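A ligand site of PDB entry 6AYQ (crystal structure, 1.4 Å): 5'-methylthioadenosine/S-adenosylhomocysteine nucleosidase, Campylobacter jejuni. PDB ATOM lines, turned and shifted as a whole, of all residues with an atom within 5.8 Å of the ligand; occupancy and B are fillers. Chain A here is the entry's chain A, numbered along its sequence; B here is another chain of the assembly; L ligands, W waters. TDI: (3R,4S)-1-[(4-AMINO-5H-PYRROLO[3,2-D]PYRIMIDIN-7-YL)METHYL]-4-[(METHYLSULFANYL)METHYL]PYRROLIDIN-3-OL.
A nitrogen (N1) of the ligand lies within hydrogen-bond range of the backbone NH (N) of Ile 162 (2.9 Å). O of Ile 162 is in hydrogen-bond range of N6 of the ligand (2.8 Å). The side-chain sulfur of Cys 180 is in hydrogen-bond range of a nitrogen (N1) of the ligand, at 3.6 Å. The side-chain carboxylate (OD2) of Asp 206 sits at hydrogen-bond distance from a nitrogen (N7) of the ligand, at 2.7 Å. An oxygen (O3') of the ligand sits at hydrogen-bond distance from the side-chain carboxylate (OE2) of Glu 183. N of Gly 88 lies close to N7 of the ligand.
The side-chain carboxylate (OD1) of Asp 206 lies within hydrogen-bond range of the backbone NH (N) of Ala 208 (3.0 Å). O of Gly 88 sits at hydrogen-bond distance from N of Cys 180, 2.8 Å away. The backbone carbonyl oxygen (O) of Ala 87 is in hydrogen-bond range of the backbone NH (N) of Ser 205, 2.9 Å away. The side-chain carboxylate (OD2) of Asp 206 is in hydrogen-bond range of the side-chain hydroxyl (OG) of Ser 205, at 2.8 Å. The side-chain carboxylate of Glu 22 is in hydrogen-bond range of the backbone NH of Ala 18, at 2.8 Å. The backbone NH of Val 86 sits at hydrogen-bond distance from the side-chain carboxylate of Glu 22 (2.9 Å). The side-chain carboxylate (OE1) of Glu 181 lies within salt-bridge range of the guanidinium group (NE) of Arg 202. The side-chain carboxylate of Glu 22 is in hydrogen-bond range of the backbone NH of Met 19 (2.8 Å).
Merely in contact with the ligand: Val 86, Ser 205, Ala 87, Phe 161, Ile 60, Glu 181, Glu 160, Ala 18, Phe 216, Phe 115 of chain B, Met 182, Ile 112 of chain B, Met 19 and Ala 208. 19 residues have an atom within 4 Å of the ligand: Ala 18, Met 19, Ile 60, Val 86, Ala 87, Gly 88, Glu 160, Phe 161, Ile 162, Cys 180, Glu 181, Met 182, Glu 183, Ser 205, Asp 206, Ala 208, Phe 216, Ile 112 of chain B and Phe 115 of chain B. Along chain A the residues within 4 Å of the ligand span positions 18 to 216.
Water W2 lies within hydrogen-bond range of OE2 of Glu 22, NH1 of Arg 202, O3' of the ligand and OE1 of Glu 183.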
ATOM      1  N   ALA A  18      -0.731  31.873  21.421  1.00  0.00           N
ATOM      2  CA  ALA A  18      -1.305  31.212  20.246  1.00  0.00           C
ATOM      3  C   ALA A  18      -2.359  32.042  19.565  1.00  0.00           C
ATOM      4  O   ALA A  18      -2.391  32.068  18.334  1.00  0.00           O
ATOM      5  CB  ALA A  18      -1.891  29.857  20.633  1.00  0.00           C
ATOM      6  N   MET A  19      -3.211  32.690  20.352  1.00  0.00           N
ATOM      7  CA  MET A  19      -4.366  33.435  19.824  1.00  0.00           C
ATOM      8  C   MET A  19      -4.239  34.916  20.113  1.00  0.00           C
ATOM      9  O   MET A  19      -3.579  35.317  21.075  1.00  0.00           O
ATOM     10  CB  MET A  19      -5.648  32.916  20.453  1.00  0.00           C
ATOM     11  CG  MET A  19      -5.892  31.448  20.169  1.00  0.00           C
ATOM     12  SD  MET A  19      -7.354  30.805  20.997  1.00  0.00           S
ATOM     13  CE  MET A  19      -8.690  31.572  20.085  1.00  0.00           C
ATOM     14  N   GLU A  22      -4.677  36.097  23.636  1.00  0.00           N
ATOM     15  CA  GLU A  22      -3.564  35.876  24.552  1.00  0.00           C
ATOM     16  C   GLU A  22      -2.475  36.950  24.495  1.00  0.00           C
ATOM     17  O   GLU A  22      -1.716  37.085  25.451  1.00  0.00           O
ATOM     18  CB  GLU A  22      -2.979  34.469  24.330  1.00  0.00           C
ATOM     19  CG  GLU A  22      -3.985  33.365  24.666  1.00  0.00           C
ATOM     20  CD  GLU A  22      -3.615  32.006  24.155  1.00  0.00           C
ATOM     21  OE1 GLU A  22      -3.015  31.912  23.077  1.00  0.00           O
ATOM     22  OE2 GLU A  22      -3.969  31.016  24.834  1.00  0.00           O
ATOM     23  N   ILE A  60      -3.132  28.770  16.144  1.00  0.00           N
ATOM     24  CA  ILE A  60      -3.315  27.587  17.000  1.00  0.00           C
ATOM     25  C   ILE A  60      -2.479  26.387  16.557  1.00  0.00           C
ATOM     26  O   ILE A  60      -2.363  26.078  15.369  1.00  0.00           O
ATOM     27  CB  ILE A  60      -4.807  27.215  17.036  1.00  0.00           C
ATOM     28  CG1 ILE A  60      -5.588  28.294  17.810  1.00  0.00           C
ATOM     29  CG2 ILE A  60      -5.027  25.848  17.664  1.00  0.00           C
ATOM     30  CD1 ILE A  60      -7.075  28.258  17.572  1.00  0.00           C
ATOM     31  N   GLY A  61      -1.912  25.690  17.550  1.00  0.00           N
ATOM     32  CA  GLY A  61      -1.368  24.353  17.324  1.00  0.00           C
ATOM     33  C   GLY A  61       0.136  24.235  17.248  1.00  0.00           C
ATOM     34  O   GLY A  61       0.881  25.221  17.300  1.00  0.00           O
ATOM     35  N   VAL A  86      -3.765  30.345  27.675  1.00  0.00           N
ATOM     36  CA  VAL A  86      -4.706  29.603  28.500  1.00  0.00           C
ATOM     37  C   VAL A  86      -4.529  28.110  28.303  1.00  0.00           C
ATOM     38  O   VAL A  86      -3.817  27.681  27.397  1.00  0.00           O
ATOM     39  CB  VAL A  86      -6.170  30.066  28.258  1.00  0.00           C
ATOM     40  CG1 VAL A  86      -6.275  31.560  28.529  1.00  0.00           C
ATOM     41  CG2 VAL A  86      -6.651  29.728  26.847  1.00  0.00           C
ATOM     42  N   ALA A  87      -5.177  27.307  29.141  1.00  0.00           N
ATOM     43  CA  ALA A  87      -5.086  25.841  29.045  1.00  0.00           C
ATOM     44  C   ALA A  87      -6.317  25.164  29.610  1.00  0.00           C
ATOM     45  O   ALA A  87      -7.134  25.787  30.300  1.00  0.00           O
ATOM     46  CB  ALA A  87      -3.825  25.334  29.735  1.00  0.00           C
ATOM     47  N   GLY A  88      -6.442  23.871  29.297  1.00  0.00           N
ATOM     48  CA  GLY A  88      -7.453  23.014  29.871  1.00  0.00           C
ATOM     49  C   GLY A  88      -6.935  22.305  31.100  1.00  0.00           C
ATOM     50  O   GLY A  88      -5.929  21.610  31.042  1.00  0.00           O
ATOM     51  N   TYR A 108       1.450  14.460  23.616  1.00  0.00           N
ATOM     52  CA  TYR A 108       0.653  13.237  23.829  1.00  0.00           C
ATOM     53  C   TYR A 108       0.191  12.558  22.563  1.00  0.00           C
ATOM     54  O   TYR A 108      -0.176  11.392  22.590  1.00  0.00           O
ATOM     55  CB  TYR A 108      -0.563  13.479  24.754  1.00  0.00           C
ATOM     56  CG  TYR A 108      -1.620  14.397  24.186  1.00  0.00           C
ATOM     57  CD1 TYR A 108      -2.523  13.953  23.210  1.00  0.00           C
ATOM     58  CD2 TYR A 108      -1.723  15.717  24.619  1.00  0.00           C
ATOM     59  CE1 TYR A 108      -3.469  14.810  22.671  1.00  0.00           C
ATOM     60  CE2 TYR A 108      -2.669  16.574  24.081  1.00  0.00           C
ATOM     61  CZ  TYR A 108      -3.554  16.112  23.126  1.00  0.00           C
ATOM     62  OH  TYR A 108      -4.454  16.992  22.569  1.00  0.00           O
ATOM     63  N   GLY A 158      -0.892  18.698  22.400  1.00  0.00           N
ATOM     64  CA  GLY A 158      -1.266  17.966  21.202  1.00  0.00           C
ATOM     65  C   GLY A 158      -2.168  18.834  20.350  1.00  0.00           C
ATOM     66  O   GLY A 158      -2.572  19.912  20.793  1.00  0.00           O
ATOM     67  N   GLU A 160      -5.272  18.662  19.386  1.00  0.00           N
ATOM     68  CA  GLU A 160      -6.702  18.536  19.588  1.00  0.00           C
ATOM     69  C   GLU A 160      -7.168  19.418  20.733  1.00  0.00           C
ATOM     70  O   GLU A 160      -6.508  19.499  21.761  1.00  0.00           O
ATOM     71  CB  GLU A 160      -7.066  17.068  19.861  1.00  0.00           C
ATOM     72  CG  GLU A 160      -8.557  16.804  20.000  1.00  0.00           C
ATOM     73  CD  GLU A 160      -8.878  15.340  20.231  1.00  0.00           C
ATOM     74  OE1 GLU A 160      -8.011  14.469  20.067  1.00  0.00           O
ATOM     75  OE2 GLU A 160     -10.045  15.067  20.574  1.00  0.00           O
ATOM     76  N   PHE A 161      -8.308  20.067  20.554  1.00  0.00           N
ATOM     77  CA  PHE A 161      -9.006  20.686  21.659  1.00  0.00           C
ATOM     78  C   PHE A 161      -9.698  19.575  22.442  1.00  0.00           C
ATOM     79  O   PHE A 161     -10.626  18.935  21.915  1.00  0.00           O
ATOM     80  CB  PHE A 161     -10.024  21.737  21.198  1.00  0.00           C
ATOM     81  CG  PHE A 161     -10.731  22.407  22.344  1.00  0.00           C
ATOM     82  CD1 PHE A 161     -10.120  23.430  23.046  1.00  0.00           C
ATOM     83  CD2 PHE A 161     -12.000  21.979  22.763  1.00  0.00           C
ATOM     84  CE1 PHE A 161     -10.758  24.043  24.115  1.00  0.00           C
ATOM     85  CE2 PHE A 161     -12.630  22.586  23.836  1.00  0.00           C
ATOM     86  CZ  PHE A 161     -12.002  23.599  24.511  1.00  0.00           C
ATOM     87  N   ILE A 162      -9.244  19.329  23.675  1.00  0.00           N
ATOM     88  CA  ILE A 162      -9.741  18.209  24.481  1.00  0.00           C
ATOM     89  C   ILE A 162     -11.023  18.620  25.206  1.00  0.00           C
ATOM     90  O   ILE A 162     -11.059  19.605  25.953  1.00  0.00           O
ATOM     91  CB  ILE A 162      -8.671  17.711  25.482  1.00  0.00           C
ATOM     92  CG1 ILE A 162      -7.391  17.275  24.757  1.00  0.00           C
ATOM     93  CG2 ILE A 162      -9.220  16.565  26.351  1.00  0.00           C
ATOM     94  CD1 ILE A 162      -7.512  16.056  23.886  1.00  0.00           C
ATOM     95  N   CYS A 163     -12.086  17.848  24.975  1.00  0.00           N
ATOM     96  CA  CYS A 163     -13.374  18.098  25.622  1.00  0.00           C
ATOM     97  C   CYS A 163     -14.062  16.756  25.814  1.00  0.00           C
ATOM     98  O   CYS A 163     -15.198  16.535  25.399  1.00  0.00           O
ATOM     99  CB  CYS A 163     -14.204  19.082  24.798  1.00  0.00           C
ATOM    100  SG  CYS A 163     -14.400  18.650  23.048  1.00  0.00           S
ATOM    101  N   CYS A 180      -3.695  20.508  29.683  1.00  0.00           N
ATOM    102  CA  CYS A 180      -3.419  20.313  28.266  1.00  0.00           C
ATOM    103  C   CYS A 180      -3.517  21.615  27.493  1.00  0.00           C
ATOM    104  O   CYS A 180      -4.184  22.561  27.897  1.00  0.00           O
ATOM    105  CB  CYS A 180      -4.353  19.282  27.648  1.00  0.00           C
ATOM    106  SG  CYS A 180      -6.099  19.782  27.584  1.00  0.00           S
ATOM    107  N   GLU A 181      -2.817  21.648  26.363  1.00  0.00           N
ATOM    108  CA  GLU A 181      -2.883  22.779  25.431  1.00  0.00           C
ATOM    109  C   GLU A 181      -2.301  22.325  24.090  1.00  0.00           C
ATOM    110  O   GLU A 181      -2.084  21.124  23.900  1.00  0.00           O
ATOM    111  CB  GLU A 181      -2.299  24.071  26.055  1.00  0.00           C
ATOM    112  CG  GLU A 181      -1.097  23.910  26.963  1.00  0.00           C
ATOM    113  CD  GLU A 181       0.212  23.862  26.232  1.00  0.00           C
ATOM    114  OE1 GLU A 181       1.151  24.558  26.722  1.00  0.00           O
ATOM    115  OE2 GLU A 181       0.291  23.160  25.185  1.00  0.00           O
ATOM    116  N   MET A 182      -2.101  23.230  23.136  1.00  0.00           N
ATOM    117  CA  MET A 182      -1.766  22.832  21.756  1.00  0.00           C
ATOM    118  C   MET A 182      -0.475  23.453  21.234  1.00  0.00           C
ATOM    119  O   MET A 182      -0.187  23.342  20.045  1.00  0.00           O
ATOM    120  CB  MET A 182      -2.973  23.173  20.827  1.00  0.00           C
ATOM    121  CG  MET A 182      -4.275  22.536  21.289  1.00  0.00           C
ATOM    122  SD  MET A 182      -5.756  23.072  20.385  1.00  0.00           S
ATOM    123  CE  MET A 182      -5.388  22.388  18.789  1.00  0.00           C
ATOM    124  N   GLU A 183       0.349  24.016  22.123  1.00  0.00           N
ATOM    125  CA  GLU A 183       1.546  24.756  21.714  1.00  0.00           C
ATOM    126  C   GLU A 183       2.761  24.644  22.632  1.00  0.00           C
ATOM    127  O   GLU A 183       3.859  24.984  22.195  1.00  0.00           O
ATOM    128  CB  GLU A 183       1.247  26.262  21.581  1.00  0.00           C
ATOM    129  CG  GLU A 183       0.095  26.618  20.629  1.00  0.00           C
ATOM    130  CD  GLU A 183      -1.320  26.508  21.192  1.00  0.00           C
ATOM    131  OE1 GLU A 183      -1.544  26.391  22.431  1.00  0.00           O
ATOM    132  OE2 GLU A 183      -2.251  26.525  20.347  1.00  0.00           O
ATOM    133  N   ARG A 202       0.422  29.124  31.735  1.00  0.00           N
ATOM    134  CA  ARG A 202      -0.965  28.979  31.292  1.00  0.00           C
ATOM    135  C   ARG A 202      -1.947  29.310  32.420  1.00  0.00           C
ATOM    136  O   ARG A 202      -1.778  28.856  33.548  1.00  0.00           O
ATOM    137  CB  ARG A 202      -1.215  27.550  30.800  1.00  0.00           C
ATOM    138  CG  ARG A 202      -0.347  27.104  29.628  1.00  0.00           C
ATOM    139  CD  ARG A 202      -0.681  27.832  28.340  1.00  0.00           C
ATOM    140  NE  ARG A 202      -0.156  27.141  27.153  1.00  0.00           N
ATOM    141  CZ  ARG A 202      -0.637  27.299  25.915  1.00  0.00           C
ATOM    142  NH1 ARG A 202      -1.669  28.108  25.681  1.00  0.00           N
ATOM    143  NH2 ARG A 202      -0.065  26.658  24.909  1.00  0.00           N
ATOM    144  N   SER A 205      -8.640  28.059  31.320  1.00  0.00           N
ATOM    145  CA  SER A 205      -9.890  28.546  30.696  1.00  0.00           C
ATOM    146  C   SER A 205     -11.061  27.564  30.790  1.00  0.00           C
ATOM    147  O   SER A 205     -12.207  27.936  30.477  1.00  0.00           O
ATOM    148  CB  SER A 205      -9.637  28.866  29.228  1.00  0.00           C
ATOM    149  OG  SER A 205      -9.134  27.728  28.534  1.00  0.00           O
ATOM    150  N   ASP A 206     -10.791  26.319  31.151  1.00  0.00           N
ATOM    151  CA  ASP A 206     -11.793  25.242  31.106  1.00  0.00           C
ATOM    152  C   ASP A 206     -11.201  23.999  31.753  1.00  0.00           C
ATOM    153  O   ASP A 206     -10.029  24.023  32.178  1.00  0.00           O
ATOM    154  CB  ASP A 206     -12.245  24.946  29.656  1.00  0.00           C
ATOM    155  CG  ASP A 206     -11.092  24.502  28.767  1.00  0.00           C
ATOM    156  OD1 ASP A 206     -10.823  23.280  28.726  1.00  0.00           O
ATOM    157  OD2 ASP A 206     -10.494  25.374  28.102  1.00  0.00           O
ATOM    158  N   LYS A 207     -11.992  22.946  31.873  1.00  0.00           N
ATOM    159  CA  LYS A 207     -11.567  21.709  32.513  1.00  0.00           C
ATOM    160  C   LYS A 207     -11.496  20.508  31.561  1.00  0.00           C
ATOM    161  O   LYS A 207     -11.453  19.360  31.987  1.00  0.00           O
ATOM    162  CB  LYS A 207     -12.454  21.439  33.750  1.00  0.00           C
ATOM    163  CG  LYS A 207     -12.269  22.499  34.839  1.00  0.00           C
ATOM    164  CD  LYS A 207     -12.918  22.105  36.160  1.00  0.00           C
ATOM    165  CE  LYS A 207     -12.783  23.207  37.190  1.00  0.00           C
ATOM    166  NZ  LYS A 207     -13.209  22.731  38.538  1.00  0.00           N
ATOM    167  N   ALA A 208     -11.453  20.792  30.258  1.00  0.00           N
ATOM    168  CA  ALA A 208     -11.140  19.798  29.230  1.00  0.00           C
ATOM    169  C   ALA A 208     -12.042  18.570  29.201  1.00  0.00           C
ATOM    170  O   ALA A 208     -11.643  17.521  28.721  1.00  0.00           O
ATOM    171  CB  ALA A 208      -9.677  19.387  29.369  1.00  0.00           C
ATOM    172  N   ALA A 212     -16.414  21.675  27.479  1.00  0.00           N
ATOM    173  CA  ALA A 212     -15.228  22.524  27.674  1.00  0.00           C
ATOM    174  C   ALA A 212     -15.153  23.675  26.667  1.00  0.00           C
ATOM    175  O   ALA A 212     -14.603  24.732  26.979  1.00  0.00           O
ATOM    176  CB  ALA A 212     -13.957  21.680  27.625  1.00  0.00           C
ATOM    177  N   PHE A 216     -14.346  27.486  27.601  1.00  0.00           N
ATOM    178  CA  PHE A 216     -13.261  28.177  26.892  1.00  0.00           C
ATOM    179  C   PHE A 216     -13.757  29.522  26.350  1.00  0.00           C
ATOM    180  O   PHE A 216     -13.143  30.546  26.606  1.00  0.00           O
ATOM    181  CB  PHE A 216     -12.699  27.321  25.732  1.00  0.00           C
ATOM    182  CG  PHE A 216     -11.748  28.082  24.877  1.00  0.00           C
ATOM    183  CD1 PHE A 216     -10.419  28.233  25.256  1.00  0.00           C
ATOM    184  CD2 PHE A 216     -12.173  28.720  23.713  1.00  0.00           C
ATOM    185  CE1 PHE A 216      -9.545  28.983  24.487  1.00  0.00           C
ATOM    186  CE2 PHE A 216     -11.305  29.459  22.938  1.00  0.00           C
ATOM    187  CZ  PHE A 216      -9.975  29.601  23.333  1.00  0.00           C
ATOM    188  N   ILE B 112      -9.864  21.235  15.948  1.00  0.00           N
ATOM    189  CA  ILE B 112     -10.645  22.119  16.828  1.00  0.00           C
ATOM    190  C   ILE B 112     -12.114  22.070  16.398  1.00  0.00           C
ATOM    191  O   ILE B 112     -12.855  23.077  16.453  1.00  0.00           O
ATOM    192  CB  ILE B 112     -10.046  23.545  16.899  1.00  0.00           C
ATOM    193  CG1 ILE B 112     -10.024  24.254  15.522  1.00  0.00           C
ATOM    194  CG2 ILE B 112      -8.620  23.470  17.463  1.00  0.00           C
ATOM    195  CD1 ILE B 112      -9.892  25.757  15.644  1.00  0.00           C
ATOM    196  N   PHE B 115     -15.490  23.503  18.033  1.00  0.00           N
ATOM    197  CA  PHE B 115     -15.984  24.861  17.786  1.00  0.00           C
ATOM    198  C   PHE B 115     -16.706  25.007  16.452  1.00  0.00           C
ATOM    199  O   PHE B 115     -17.131  26.113  16.111  1.00  0.00           O
ATOM    200  CB  PHE B 115     -14.831  25.856  17.884  1.00  0.00           C
ATOM    201  CG  PHE B 115     -14.193  25.892  19.244  1.00  0.00           C
ATOM    202  CD1 PHE B 115     -14.794  26.573  20.295  1.00  0.00           C
ATOM    203  CD2 PHE B 115     -13.009  25.197  19.493  1.00  0.00           C
ATOM    204  CE1 PHE B 115     -14.230  26.587  21.558  1.00  0.00           C
ATOM    205  CE2 PHE B 115     -12.440  25.219  20.753  1.00  0.00           C
ATOM    206  CZ  PHE B 115     -13.041  25.904  21.780  1.00  0.00           C
HETATM  207  C2  TDI L   1      -6.661  21.985  24.235  1.00  0.00           C
HETATM  208  C4  TDI L   1      -6.715  24.067  25.196  1.00  0.00           C
HETATM  209  C5  TDI L   1      -7.881  23.694  25.978  1.00  0.00           C
HETATM  210  C6  TDI L   1      -8.376  22.333  25.807  1.00  0.00           C
HETATM  211  CS5 TDI L   1      -9.648  27.301  19.983  1.00  0.00           C
HETATM  212  S   TDI L   1      -8.636  25.862  20.230  1.00  0.00           S
HETATM  213  C5' TDI L   1      -8.016  26.220  21.856  1.00  0.00           C
HETATM  214  C4' TDI L   1      -6.840  27.207  21.882  1.00  0.00           C
HETATM  215  C1' TDI L   1      -6.501  27.655  23.293  1.00  0.00           C
HETATM  216  N1' TDI L   1      -5.533  26.641  23.687  1.00  0.00           N
HETATM  217  C10 TDI L   1      -5.266  26.349  25.069  1.00  0.00           C
HETATM  218  C9  TDI L   1      -6.392  25.457  25.536  1.00  0.00           C
HETATM  219  C8  TDI L   1      -7.353  25.800  26.471  1.00  0.00           C
HETATM  220  N7  TDI L   1      -8.223  24.774  26.705  1.00  0.00           N
HETATM  221  N6  TDI L   1      -9.441  21.882  26.491  1.00  0.00           N
HETATM  222  N1  TDI L   1      -7.749  21.540  24.924  1.00  0.00           N
HETATM  223  N3  TDI L   1      -6.125  23.204  24.332  1.00  0.00           N
HETATM  224  C2' TDI L   1      -4.976  25.890  22.577  1.00  0.00           C
HETATM  225  C3' TDI L   1      -5.527  26.623  21.377  1.00  0.00           C
HETATM  226  O3' TDI L   1      -4.616  27.660  21.053  1.00  0.00           O
HETATM  227  O   HOH W   1      -4.455  19.447  23.601  1.00  0.00           O
HETATM  228  O   HOH W   2      -3.459  28.728  23.614  1.00  0.00           O
